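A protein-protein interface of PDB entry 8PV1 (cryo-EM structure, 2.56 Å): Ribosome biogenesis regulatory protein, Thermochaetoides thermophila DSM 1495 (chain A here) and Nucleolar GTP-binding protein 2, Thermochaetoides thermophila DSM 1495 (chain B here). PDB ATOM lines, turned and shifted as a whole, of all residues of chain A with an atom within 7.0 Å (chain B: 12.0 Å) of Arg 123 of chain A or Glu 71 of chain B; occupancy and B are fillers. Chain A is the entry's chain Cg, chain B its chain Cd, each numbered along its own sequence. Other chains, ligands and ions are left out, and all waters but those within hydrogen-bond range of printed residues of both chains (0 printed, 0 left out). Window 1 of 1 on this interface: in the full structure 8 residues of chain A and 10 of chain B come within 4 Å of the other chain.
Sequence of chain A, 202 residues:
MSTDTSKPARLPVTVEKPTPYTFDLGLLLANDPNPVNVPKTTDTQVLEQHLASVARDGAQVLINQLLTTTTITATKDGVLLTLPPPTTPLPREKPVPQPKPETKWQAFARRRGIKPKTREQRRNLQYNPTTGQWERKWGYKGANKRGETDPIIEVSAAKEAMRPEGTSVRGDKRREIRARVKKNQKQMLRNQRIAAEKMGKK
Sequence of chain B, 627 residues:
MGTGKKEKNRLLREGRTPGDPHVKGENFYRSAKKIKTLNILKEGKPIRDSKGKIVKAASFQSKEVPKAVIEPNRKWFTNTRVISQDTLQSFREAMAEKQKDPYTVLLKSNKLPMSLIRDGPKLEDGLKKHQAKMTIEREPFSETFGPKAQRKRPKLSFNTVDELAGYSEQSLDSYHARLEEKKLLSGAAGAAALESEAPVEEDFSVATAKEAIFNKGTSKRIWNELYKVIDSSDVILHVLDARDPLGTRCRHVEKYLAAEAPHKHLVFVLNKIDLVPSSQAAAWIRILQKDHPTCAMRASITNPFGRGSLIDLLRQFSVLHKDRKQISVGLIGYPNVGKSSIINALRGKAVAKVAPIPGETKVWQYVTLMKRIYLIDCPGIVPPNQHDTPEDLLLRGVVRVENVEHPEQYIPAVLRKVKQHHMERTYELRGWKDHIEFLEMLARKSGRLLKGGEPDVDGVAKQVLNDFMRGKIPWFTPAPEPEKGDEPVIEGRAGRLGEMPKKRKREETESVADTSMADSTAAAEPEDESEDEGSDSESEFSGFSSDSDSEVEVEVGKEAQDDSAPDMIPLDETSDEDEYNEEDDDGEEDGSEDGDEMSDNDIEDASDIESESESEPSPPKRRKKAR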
ATOM      1  N   LYS A 117     -15.180 -28.590  35.963  1.00  0.00           N
ATOM      2  CA  LYS A 117     -15.978 -28.251  34.795  1.00  0.00           C
ATOM      3  C   LYS A 117     -15.105 -28.212  33.548  1.00  0.00           C
ATOM      4  O   LYS A 117     -13.945 -27.795  33.588  1.00  0.00           O
ATOM      5  CB  LYS A 117     -16.668 -26.902  34.994  1.00  0.00           C
ATOM      6  CG  LYS A 117     -17.833 -26.937  35.966  1.00  0.00           C
ATOM      7  CD  LYS A 117     -17.952 -25.641  36.749  1.00  0.00           C
ATOM      8  CE  LYS A 117     -18.027 -24.434  35.837  1.00  0.00           C
ATOM      9  NZ  LYS A 117     -17.927 -23.168  36.610  1.00  0.00           N
ATOM     10  N   THR A 118     -15.672 -28.657  32.433  1.00  0.00           N
ATOM     11  CA  THR A 118     -14.941 -28.639  31.177  1.00  0.00           C
ATOM     12  C   THR A 118     -14.821 -27.212  30.653  1.00  0.00           C
ATOM     13  O   THR A 118     -15.563 -26.310  31.055  1.00  0.00           O
ATOM     14  CB  THR A 118     -15.623 -29.529  30.136  1.00  0.00           C
ATOM     15  OG1 THR A 118     -16.855 -28.934  29.719  1.00  0.00           O
ATOM     16  CG2 THR A 118     -15.905 -30.902  30.715  1.00  0.00           C
ATOM     17  N   ARG A 119     -13.856 -27.017  29.750  1.00  0.00           N
ATOM     18  CA  ARG A 119     -13.578 -25.684  29.229  1.00  0.00           C
ATOM     19  C   ARG A 119     -14.721 -25.162  28.373  1.00  0.00           C
ATOM     20  O   ARG A 119     -14.924 -23.948  28.288  1.00  0.00           O
ATOM     21  CB  ARG A 119     -12.276 -25.697  28.432  1.00  0.00           C
ATOM     22  CG  ARG A 119     -11.067 -26.116  29.244  1.00  0.00           C
ATOM     23  CD  ARG A 119      -9.801 -26.060  28.415  1.00  0.00           C
ATOM     24  NE  ARG A 119      -9.413 -24.687  28.123  1.00  0.00           N
ATOM     25  CZ  ARG A 119      -8.521 -23.997  28.818  1.00  0.00           C
ATOM     26  NH1 ARG A 119      -7.890 -24.528  29.852  1.00  0.00           N
ATOM     27  NH2 ARG A 119      -8.254 -22.743  28.467  1.00  0.00           N
ATOM     28  N   GLU A 120     -15.474 -26.057  27.733  1.00  0.00           N
ATOM     29  CA  GLU A 120     -16.666 -25.631  27.009  1.00  0.00           C
ATOM     30  C   GLU A 120     -17.788 -25.268  27.974  1.00  0.00           C
ATOM     31  O   GLU A 120     -18.537 -24.313  27.736  1.00  0.00           O
ATOM     32  CB  GLU A 120     -17.111 -26.730  26.040  1.00  0.00           C
ATOM     33  CG  GLU A 120     -18.458 -26.500  25.344  1.00  0.00           C
ATOM     34  CD  GLU A 120     -18.446 -25.390  24.294  1.00  0.00           C
ATOM     35  OE1 GLU A 120     -19.521 -25.125  23.715  1.00  0.00           O
ATOM     36  OE2 GLU A 120     -17.378 -24.804  24.014  1.00  0.00           O
ATOM     37  N   GLN A 121     -17.908 -26.012  29.073  1.00  0.00           N
ATOM     38  CA  GLN A 121     -18.938 -25.743  30.067  1.00  0.00           C
ATOM     39  C   GLN A 121     -18.708 -24.424  30.794  1.00  0.00           C
ATOM     40  O   GLN A 121     -19.678 -23.732  31.121  1.00  0.00           O
ATOM     41  CB  GLN A 121     -18.994 -26.905  31.062  1.00  0.00           C
ATOM     42  CG  GLN A 121     -19.999 -26.767  32.183  1.00  0.00           C
ATOM     43  CD  GLN A 121     -19.950 -27.940  33.138  1.00  0.00           C
ATOM     44  OE1 GLN A 121     -19.198 -28.891  32.932  1.00  0.00           O
ATOM     45  NE2 GLN A 121     -20.755 -27.880  34.192  1.00  0.00           N
ATOM     46  N   ARG A 122     -17.454 -24.047  31.030  1.00  0.00           N
ATOM     47  CA  ARG A 122     -17.146 -22.839  31.784  1.00  0.00           C
ATOM     48  C   ARG A 122     -16.930 -21.614  30.899  1.00  0.00           C
ATOM     49  O   ARG A 122     -16.369 -20.618  31.368  1.00  0.00           O
ATOM     50  CB  ARG A 122     -15.922 -23.073  32.672  1.00  0.00           C
ATOM     51  CG  ARG A 122     -14.618 -23.252  31.924  1.00  0.00           C
ATOM     52  CD  ARG A 122     -13.580 -23.910  32.799  1.00  0.00           C
ATOM     53  NE  ARG A 122     -12.240 -23.758  32.251  1.00  0.00           N
ATOM     54  CZ  ARG A 122     -11.172 -24.395  32.707  1.00  0.00           C
ATOM     55  NH1 ARG A 122     -11.253 -25.244  33.717  1.00  0.00           N
ATOM     56  NH2 ARG A 122      -9.992 -24.171  32.137  1.00  0.00           N
ATOM     57  N   ARG A 123     -17.372 -21.652  29.644  1.00  0.00           N
ATOM     58  CA  ARG A 123     -17.215 -20.509  28.754  1.00  0.00           C
ATOM     59  C   ARG A 123     -18.092 -19.341  29.190  1.00  0.00           C
ATOM     60  O   ARG A 123     -19.181 -19.519  29.742  1.00  0.00           O
ATOM     61  CB  ARG A 123     -17.565 -20.889  27.317  1.00  0.00           C
ATOM     62  CG  ARG A 123     -16.487 -21.661  26.594  1.00  0.00           C
ATOM     63  CD  ARG A 123     -16.759 -21.694  25.106  1.00  0.00           C
ATOM     64  NE  ARG A 123     -16.824 -20.352  24.542  1.00  0.00           N
ATOM     65  CZ  ARG A 123     -17.267 -20.071  23.325  1.00  0.00           C
ATOM     66  NH1 ARG A 123     -17.723 -21.017  22.521  1.00  0.00           N
ATOM     67  NH2 ARG A 123     -17.250 -18.811  22.903  1.00  0.00           N
ATOM     68  N   ASN A 124     -17.602 -18.128  28.928  1.00  0.00           N
ATOM     69  CA  ASN A 124     -18.343 -16.901  29.224  1.00  0.00           C
ATOM     70  C   ASN A 124     -19.208 -16.536  28.018  1.00  0.00           C
ATOM     71  O   ASN A 124     -19.005 -15.530  27.334  1.00  0.00           O
ATOM     72  CB  ASN A 124     -17.388 -15.776  29.590  1.00  0.00           C
ATOM     73  CG  ASN A 124     -18.104 -14.554  30.129  1.00  0.00           C
ATOM     74  OD1 ASN A 124     -19.277 -14.618  30.491  1.00  0.00           O
ATOM     75  ND2 ASN A 124     -17.402 -13.430  30.175  1.00  0.00           N
ATOM     76  N   LEU A 125     -20.197 -17.388  27.760  1.00  0.00           N
ATOM     77  CA  LEU A 125     -21.094 -17.190  26.633  1.00  0.00           C
ATOM     78  C   LEU A 125     -22.363 -17.993  26.864  1.00  0.00           C
ATOM     79  O   LEU A 125     -22.308 -19.130  27.333  1.00  0.00           O
ATOM     80  CB  LEU A 125     -20.441 -17.614  25.312  1.00  0.00           C
ATOM     81  CG  LEU A 125     -21.107 -17.078  24.046  1.00  0.00           C
ATOM     82  CD1 LEU A 125     -21.058 -15.559  24.011  1.00  0.00           C
ATOM     83  CD2 LEU A 125     -20.462 -17.668  22.808  1.00  0.00           C
ATOM     84  N   GLN A 126     -23.500 -17.390  26.531  1.00  0.00           N
ATOM     85  CA  GLN A 126     -24.778 -18.080  26.584  1.00  0.00           C
ATOM     86  C   GLN A 126     -25.690 -17.464  25.538  1.00  0.00           C
ATOM     87  O   GLN A 126     -25.469 -16.336  25.091  1.00  0.00           O
ATOM     88  CB  GLN A 126     -25.416 -17.995  27.973  1.00  0.00           C
ATOM     89  CG  GLN A 126     -25.825 -16.594  28.382  1.00  0.00           C
ATOM     90  CD  GLN A 126     -26.493 -16.561  29.739  1.00  0.00           C
ATOM     91  OE1 GLN A 126     -26.383 -17.505  30.520  1.00  0.00           O
ATOM     92  NE2 GLN A 126     -27.194 -15.475  30.025  1.00  0.00           N
ATOM     93  N   TRP A 134     -26.399 -13.919  21.325  1.00  0.00           N
ATOM     94  CA  TRP A 134     -25.399 -14.467  22.227  1.00  0.00           C
ATOM     95  C   TRP A 134     -24.883 -13.373  23.149  1.00  0.00           C
ATOM     96  O   TRP A 134     -24.601 -12.255  22.709  1.00  0.00           O
ATOM     97  CB  TRP A 134     -24.243 -15.086  21.442  1.00  0.00           C
ATOM     98  CG  TRP A 134     -24.620 -16.345  20.737  1.00  0.00           C
ATOM     99  CD1 TRP A 134     -25.092 -16.462  19.464  1.00  0.00           C
ATOM    100  CD2 TRP A 134     -24.565 -17.671  21.268  1.00  0.00           C
ATOM    101  NE1 TRP A 134     -25.332 -17.780  19.168  1.00  0.00           N
ATOM    102  CE2 TRP A 134     -25.018 -18.543  20.262  1.00  0.00           C
ATOM    103  CE3 TRP A 134     -24.178 -18.207  22.499  1.00  0.00           C
ATOM    104  CZ2 TRP A 134     -25.089 -19.919  20.445  1.00  0.00           C
ATOM    105  CZ3 TRP A 134     -24.251 -19.574  22.680  1.00  0.00           C
ATOM    106  CH2 TRP A 134     -24.704 -20.414  21.659  1.00  0.00           C
ATOM    107  N   LYS A 137     -22.108 -14.166  30.295  1.00  0.00           N
ATOM    108  CA  LYS A 137     -22.698 -14.410  31.606  1.00  0.00           C
ATOM    109  C   LYS A 137     -22.227 -13.403  32.645  1.00  0.00           C
ATOM    110  O   LYS A 137     -22.986 -13.062  33.559  1.00  0.00           O
ATOM    111  CB  LYS A 137     -22.372 -15.826  32.079  1.00  0.00           C
ATOM    112  CG  LYS A 137     -22.721 -16.915  31.087  1.00  0.00           C
ATOM    113  CD  LYS A 137     -22.192 -18.256  31.552  1.00  0.00           C
ATOM    114  CE  LYS A 137     -22.723 -19.387  30.692  1.00  0.00           C
ATOM    115  NZ  LYS A 137     -22.080 -20.684  31.037  1.00  0.00           N
ATOM    116  N   TRP A 138     -20.991 -12.928  32.530  1.00  0.00           N
ATOM    117  CA  TRP A 138     -20.421 -12.002  33.496  1.00  0.00           C
ATOM    118  C   TRP A 138     -19.508 -11.036  32.758  1.00  0.00           C
ATOM    119  O   TRP A 138     -19.300 -11.147  31.548  1.00  0.00           O
ATOM    120  CB  TRP A 138     -19.664 -12.749  34.600  1.00  0.00           C
ATOM    121  CG  TRP A 138     -18.511 -13.554  34.091  1.00  0.00           C
ATOM    122  CD1 TRP A 138     -18.556 -14.821  33.596  1.00  0.00           C
ATOM    123  CD2 TRP A 138     -17.138 -13.152  34.036  1.00  0.00           C
ATOM    124  NE1 TRP A 138     -17.301 -15.230  33.227  1.00  0.00           N
ATOM    125  CE2 TRP A 138     -16.411 -14.224  33.489  1.00  0.00           C
ATOM    126  CE3 TRP A 138     -16.452 -11.989  34.397  1.00  0.00           C
ATOM    127  CZ2 TRP A 138     -15.037 -14.169  33.292  1.00  0.00           C
ATOM    128  CZ3 TRP A 138     -15.087 -11.936  34.200  1.00  0.00           C
ATOM    129  CH2 TRP A 138     -14.394 -13.019  33.653  1.00  0.00           C
ATOM    130  N   LYS B  67     -32.859 -25.154  22.869  1.00  0.00           N
ATOM    131  CA  LYS B  67     -32.472 -24.245  21.798  1.00  0.00           C
ATOM    132  C   LYS B  67     -31.184 -24.766  21.176  1.00  0.00           C
ATOM    133  O   LYS B  67     -30.127 -24.754  21.815  1.00  0.00           O
ATOM    134  CB  LYS B  67     -32.301 -22.827  22.332  1.00  0.00           C
ATOM    135  CG  LYS B  67     -33.612 -22.112  22.598  1.00  0.00           C
ATOM    136  CD  LYS B  67     -34.480 -22.075  21.353  1.00  0.00           C
ATOM    137  CE  LYS B  67     -35.795 -21.361  21.614  1.00  0.00           C
ATOM    138  NZ  LYS B  67     -35.595 -19.931  21.966  1.00  0.00           N
ATOM    139  N   ALA B  68     -31.271 -25.231  19.933  1.00  0.00           N
ATOM    140  CA  ALA B  68     -30.135 -25.846  19.249  1.00  0.00           C
ATOM    141  C   ALA B  68     -29.495 -24.792  18.358  1.00  0.00           C
ATOM    142  O   ALA B  68     -29.886 -24.590  17.209  1.00  0.00           O
ATOM    143  CB  ALA B  68     -30.583 -27.071  18.464  1.00  0.00           C
ATOM    144  N   VAL B  69     -28.497 -24.105  18.905  1.00  0.00           N
ATOM    145  CA  VAL B  69     -27.860 -22.961  18.264  1.00  0.00           C
ATOM    146  C   VAL B  69     -26.346 -23.125  18.312  1.00  0.00           C
ATOM    147  O   VAL B  69     -25.796 -23.662  19.280  1.00  0.00           O
ATOM    148  CB  VAL B  69     -28.302 -21.633  18.919  1.00  0.00           C
ATOM    149  CG1 VAL B  69     -29.771 -21.378  18.670  1.00  0.00           C
ATOM    150  CG2 VAL B  69     -28.104 -21.709  20.417  1.00  0.00           C
ATOM    151  N   ILE B  70     -25.677 -22.688  17.248  1.00  0.00           N
ATOM    152  CA  ILE B  70     -24.222 -22.726  17.136  1.00  0.00           C
ATOM    153  C   ILE B  70     -23.713 -21.292  17.144  1.00  0.00           C
ATOM    154  O   ILE B  70     -24.122 -20.478  16.306  1.00  0.00           O
ATOM    155  CB  ILE B  70     -23.764 -23.458  15.864  1.00  0.00           C
ATOM    156  CG1 ILE B  70     -24.358 -24.868  15.796  1.00  0.00           C
ATOM    157  CG2 ILE B  70     -22.244 -23.499  15.786  1.00  0.00           C
ATOM    158  CD1 ILE B  70     -23.697 -25.858  16.727  1.00  0.00           C
ATOM    159  N   GLU B  71     -22.822 -20.981  18.081  1.00  0.00           N
ATOM    160  CA  GLU B  71     -22.295 -19.629  18.160  1.00  0.00           C
ATOM    161  C   GLU B  71     -21.259 -19.389  17.061  1.00  0.00           C
ATOM    162  O   GLU B  71     -20.630 -20.331  16.572  1.00  0.00           O
ATOM    163  CB  GLU B  71     -21.674 -19.375  19.534  1.00  0.00           C
ATOM    164  CG  GLU B  71     -20.206 -19.750  19.678  1.00  0.00           C
ATOM    165  CD  GLU B  71     -19.996 -21.229  19.927  1.00  0.00           C
ATOM    166  OE1 GLU B  71     -20.997 -21.958  20.087  1.00  0.00           O
ATOM    167  OE2 GLU B  71     -18.827 -21.665  19.963  1.00  0.00           O
ATOM    168  N   PRO B  72     -21.108 -18.143  16.617  1.00  0.00           N
ATOM    169  CA  PRO B  72     -19.992 -17.822  15.722  1.00  0.00           C
ATOM    170  C   PRO B  72     -18.667 -17.917  16.460  1.00  0.00           C
ATOM    171  O   PRO B  72     -18.542 -17.491  17.610  1.00  0.00           O
ATOM    172  CB  PRO B  72     -20.289 -16.386  15.272  1.00  0.00           C
ATOM    173  CG  PRO B  72     -21.270 -15.861  16.259  1.00  0.00           C
ATOM    174  CD  PRO B  72     -22.066 -17.032  16.724  1.00  0.00           C
ATOM    175  N   ASN B  73     -17.672 -18.482  15.783  1.00  0.00           N
ATOM    176  CA  ASN B  73     -16.389 -18.762  16.406  1.00  0.00           C
ATOM    177  C   ASN B  73     -15.343 -18.898  15.314  1.00  0.00           C
ATOM    178  O   ASN B  73     -15.598 -19.520  14.280  1.00  0.00           O
ATOM    179  CB  ASN B  73     -16.450 -20.040  17.249  1.00  0.00           C
ATOM    180  CG  ASN B  73     -15.374 -20.098  18.310  1.00  0.00           C
ATOM    181  OD1 ASN B  73     -14.239 -19.680  18.088  1.00  0.00           O
ATOM    182  ND2 ASN B  73     -15.725 -20.630  19.472  1.00  0.00           N
ATOM    183  N   ARG B  74     -14.162 -18.326  15.558  1.00  0.00           N
ATOM    184  CA  ARG B  74     -13.085 -18.409  14.579  1.00  0.00           C
ATOM    185  C   ARG B  74     -12.508 -19.815  14.493  1.00  0.00           C
ATOM    186  O   ARG B  74     -11.841 -20.150  13.509  1.00  0.00           O
ATOM    187  CB  ARG B  74     -11.987 -17.403  14.921  1.00  0.00           C
ATOM    188  N   LYS B  75     -12.758 -20.652  15.505  1.00  0.00           N
ATOM    189  CA  LYS B  75     -12.208 -22.003  15.514  1.00  0.00           C
ATOM    190  C   LYS B  75     -12.850 -22.895  14.461  1.00  0.00           C
ATOM    191  O   LYS B  75     -12.268 -23.915  14.077  1.00  0.00           O
ATOM    192  CB  LYS B  75     -12.373 -22.628  16.902  1.00  0.00           C
ATOM    193  CG  LYS B  75     -13.786 -23.096  17.214  1.00  0.00           C
ATOM    194  CD  LYS B  75     -13.797 -24.221  18.231  1.00  0.00           C
ATOM    195  CE  LYS B  75     -13.436 -23.722  19.612  1.00  0.00           C
ATOM    196  NZ  LYS B  75     -13.648 -24.774  20.641  1.00  0.00           N
ATOM    197  N   TRP B  76     -14.041 -22.533  13.974  1.00  0.00           N
ATOM    198  CA  TRP B  76     -14.727 -23.374  13.001  1.00  0.00           C
ATOM    199  C   TRP B  76     -14.084 -23.318  11.625  1.00  0.00           C
ATOM    200  O   TRP B  76     -14.361 -24.186  10.791  1.00  0.00           O
ATOM    201  CB  TRP B  76     -16.200 -22.971  12.873  1.00  0.00           C
ATOM    202  CG  TRP B  76     -17.015 -22.921  14.148  1.00  0.00           C
ATOM    203  CD1 TRP B  76     -17.866 -21.922  14.517  1.00  0.00           C
ATOM    204  CD2 TRP B  76     -17.101 -23.918  15.183  1.00  0.00           C
ATOM    205  NE1 TRP B  76     -18.456 -22.217  15.718  1.00  0.00           N
ATOM    206  CE2 TRP B  76     -18.003 -23.434  16.149  1.00  0.00           C
ATOM    207  CE3 TRP B  76     -16.496 -25.162  15.393  1.00  0.00           C
ATOM    208  CZ2 TRP B  76     -18.313 -24.146  17.303  1.00  0.00           C
ATOM    209  CZ3 TRP B  76     -16.804 -25.863  16.539  1.00  0.00           C
ATOM    210  CH2 TRP B  76     -17.705 -25.356  17.478  1.00  0.00           C
ATOM    211  N   PHE B  77     -13.234 -22.327  11.367  1.00  0.00           N
ATOM    212  CA  PHE B  77     -12.721 -22.069  10.029  1.00  0.00           C
ATOM    213  C   PHE B  77     -11.211 -22.254   9.940  1.00  0.00           C
ATOM    214  O   PHE B  77     -10.594 -21.817   8.966  1.00  0.00           O
ATOM    215  CB  PHE B  77     -13.117 -20.662   9.580  1.00  0.00           C
ATOM    216  CG  PHE B  77     -14.604 -20.452   9.483  1.00  0.00           C
ATOM    217  CD1 PHE B  77     -15.341 -20.059  10.589  1.00  0.00           C
ATOM    218  CD2 PHE B  77     -15.266 -20.658   8.286  1.00  0.00           C
ATOM    219  CE1 PHE B  77     -16.704 -19.875  10.500  1.00  0.00           C
ATOM    220  CE2 PHE B  77     -16.629 -20.472   8.192  1.00  0.00           C
ATOM    221  CZ  PHE B  77     -17.348 -20.080   9.302  1.00  0.00           C
ATOM    222  N   THR B  78     -10.606 -22.891  10.935  1.00  0.00           N
ATOM    223  CA  THR B  78      -9.174 -23.145  10.953  1.00  0.00           C
ATOM    224  C   THR B  78      -8.895 -24.627  10.749  1.00  0.00           C
ATOM    225  O   THR B  78      -9.795 -25.471  10.782  1.00  0.00           O
ATOM    226  CB  THR B  78      -8.549 -22.668  12.270  1.00  0.00           C
ATOM    227  OG1 THR B  78      -9.023 -23.482  13.349  1.00  0.00           O
ATOM    228  CG2 THR B  78      -8.902 -21.219  12.538  1.00  0.00           C
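Of the 12 printed residues of chain B, 4 touch a printed residue of chain A. Printed residues of chain B that touch a printed residue of chain A: Val 69, Ile 70, Glu 71 and Asn 73. Hydrophobic or aromatic side chains of chain B that line the printed part of chain A: Val 69. Along chain B the printed residues that touch a printed residue of chain A span positions 69 to 73. Of the 13 printed residues of chain A, 3 touch a printed residue of chain B. Among the printed residues, 6 pairs touch across the chains. Among the printed residues, Asp or Glu carboxylates within 4 Å of a Lys or Arg side-chain nitrogen of the other chain: Arg 123 of chain A with Glu 71 of chain B (2.9 Å).
The side-chain carboxylate of Glu 71 of chain B lies within salt-bridge range of the guanidinium group of Arg 123 of chain A.
Arg 119 of chain A touches none of the printed residues of chain B. No residue of chain B comes within 4 Å of Glu 120 of chain A. Of chain B, only Glu 71 and Asn 73 come within 4 Å of Arg 123 of chain A. Of the printed residues of chain B, Trp 134 of chain A touches Val 69, Ile 70 and Glu 71. Printed residues of chain A within 4 Å of Val 69 of chain B: Trp 134. Printed residues of chain A within 4 Å of Ile 70 of chain B: Trp 134. Glu 71 of chain B touches just these residues of chain A: Arg 123 (2.9 Å), Leu 125 (3.8 Å) and Trp 134 (3.4 Å). Printed residues of chain A within 4 Å of Asn 73 of chain B: Arg 123. The nearest residue of chain B that does not touch Arg 123 of chain A is Pro 72 of chain B (5.6 Å). The nearest residue of chain A that does not touch Glu 71 of chain B is Glu 120 of chain A (5.0 Å). The nearest printed residue of chain A that does not touch Asn 73 of chain B is Glu 120 of chain A (6.4 Å).
Arg 123 of chain A touches Asn 73 of chain B. Glu 71 of chain B touches Leu 125 of chain A. Trp 134 of chain A touches Val 69 of chain B (CZ2 to CG2, 3.5 Å). Ile 70 of chain B touches Trp 134 of chain A. N of Glu 71 of chain B touches CZ2 of Trp 134 of chain A, 3.4 Å away.
The side-chain amino group (NZ) of Lys 137 of chain A is in hydrogen-bond range of the backbone carbonyl oxygen (O) of Arg 123 of chain A, at 3.4 Å. The side-chain amide nitrogen (ND2) of Asn 73 of chain B lies within hydrogen-bond range of the side-chain carboxylate (OE2) of Glu 71 of chain B (3.3 Å). N of Lys 75 of chain B lies close to OD1 of Asn 73 of chain B (3.1 Å). The indole nitrogen (NE1) of Trp 76 of chain B sits at hydrogen-bond distance from the backbone carbonyl oxygen (O) of Glu 71 of chain B (3.0 Å).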
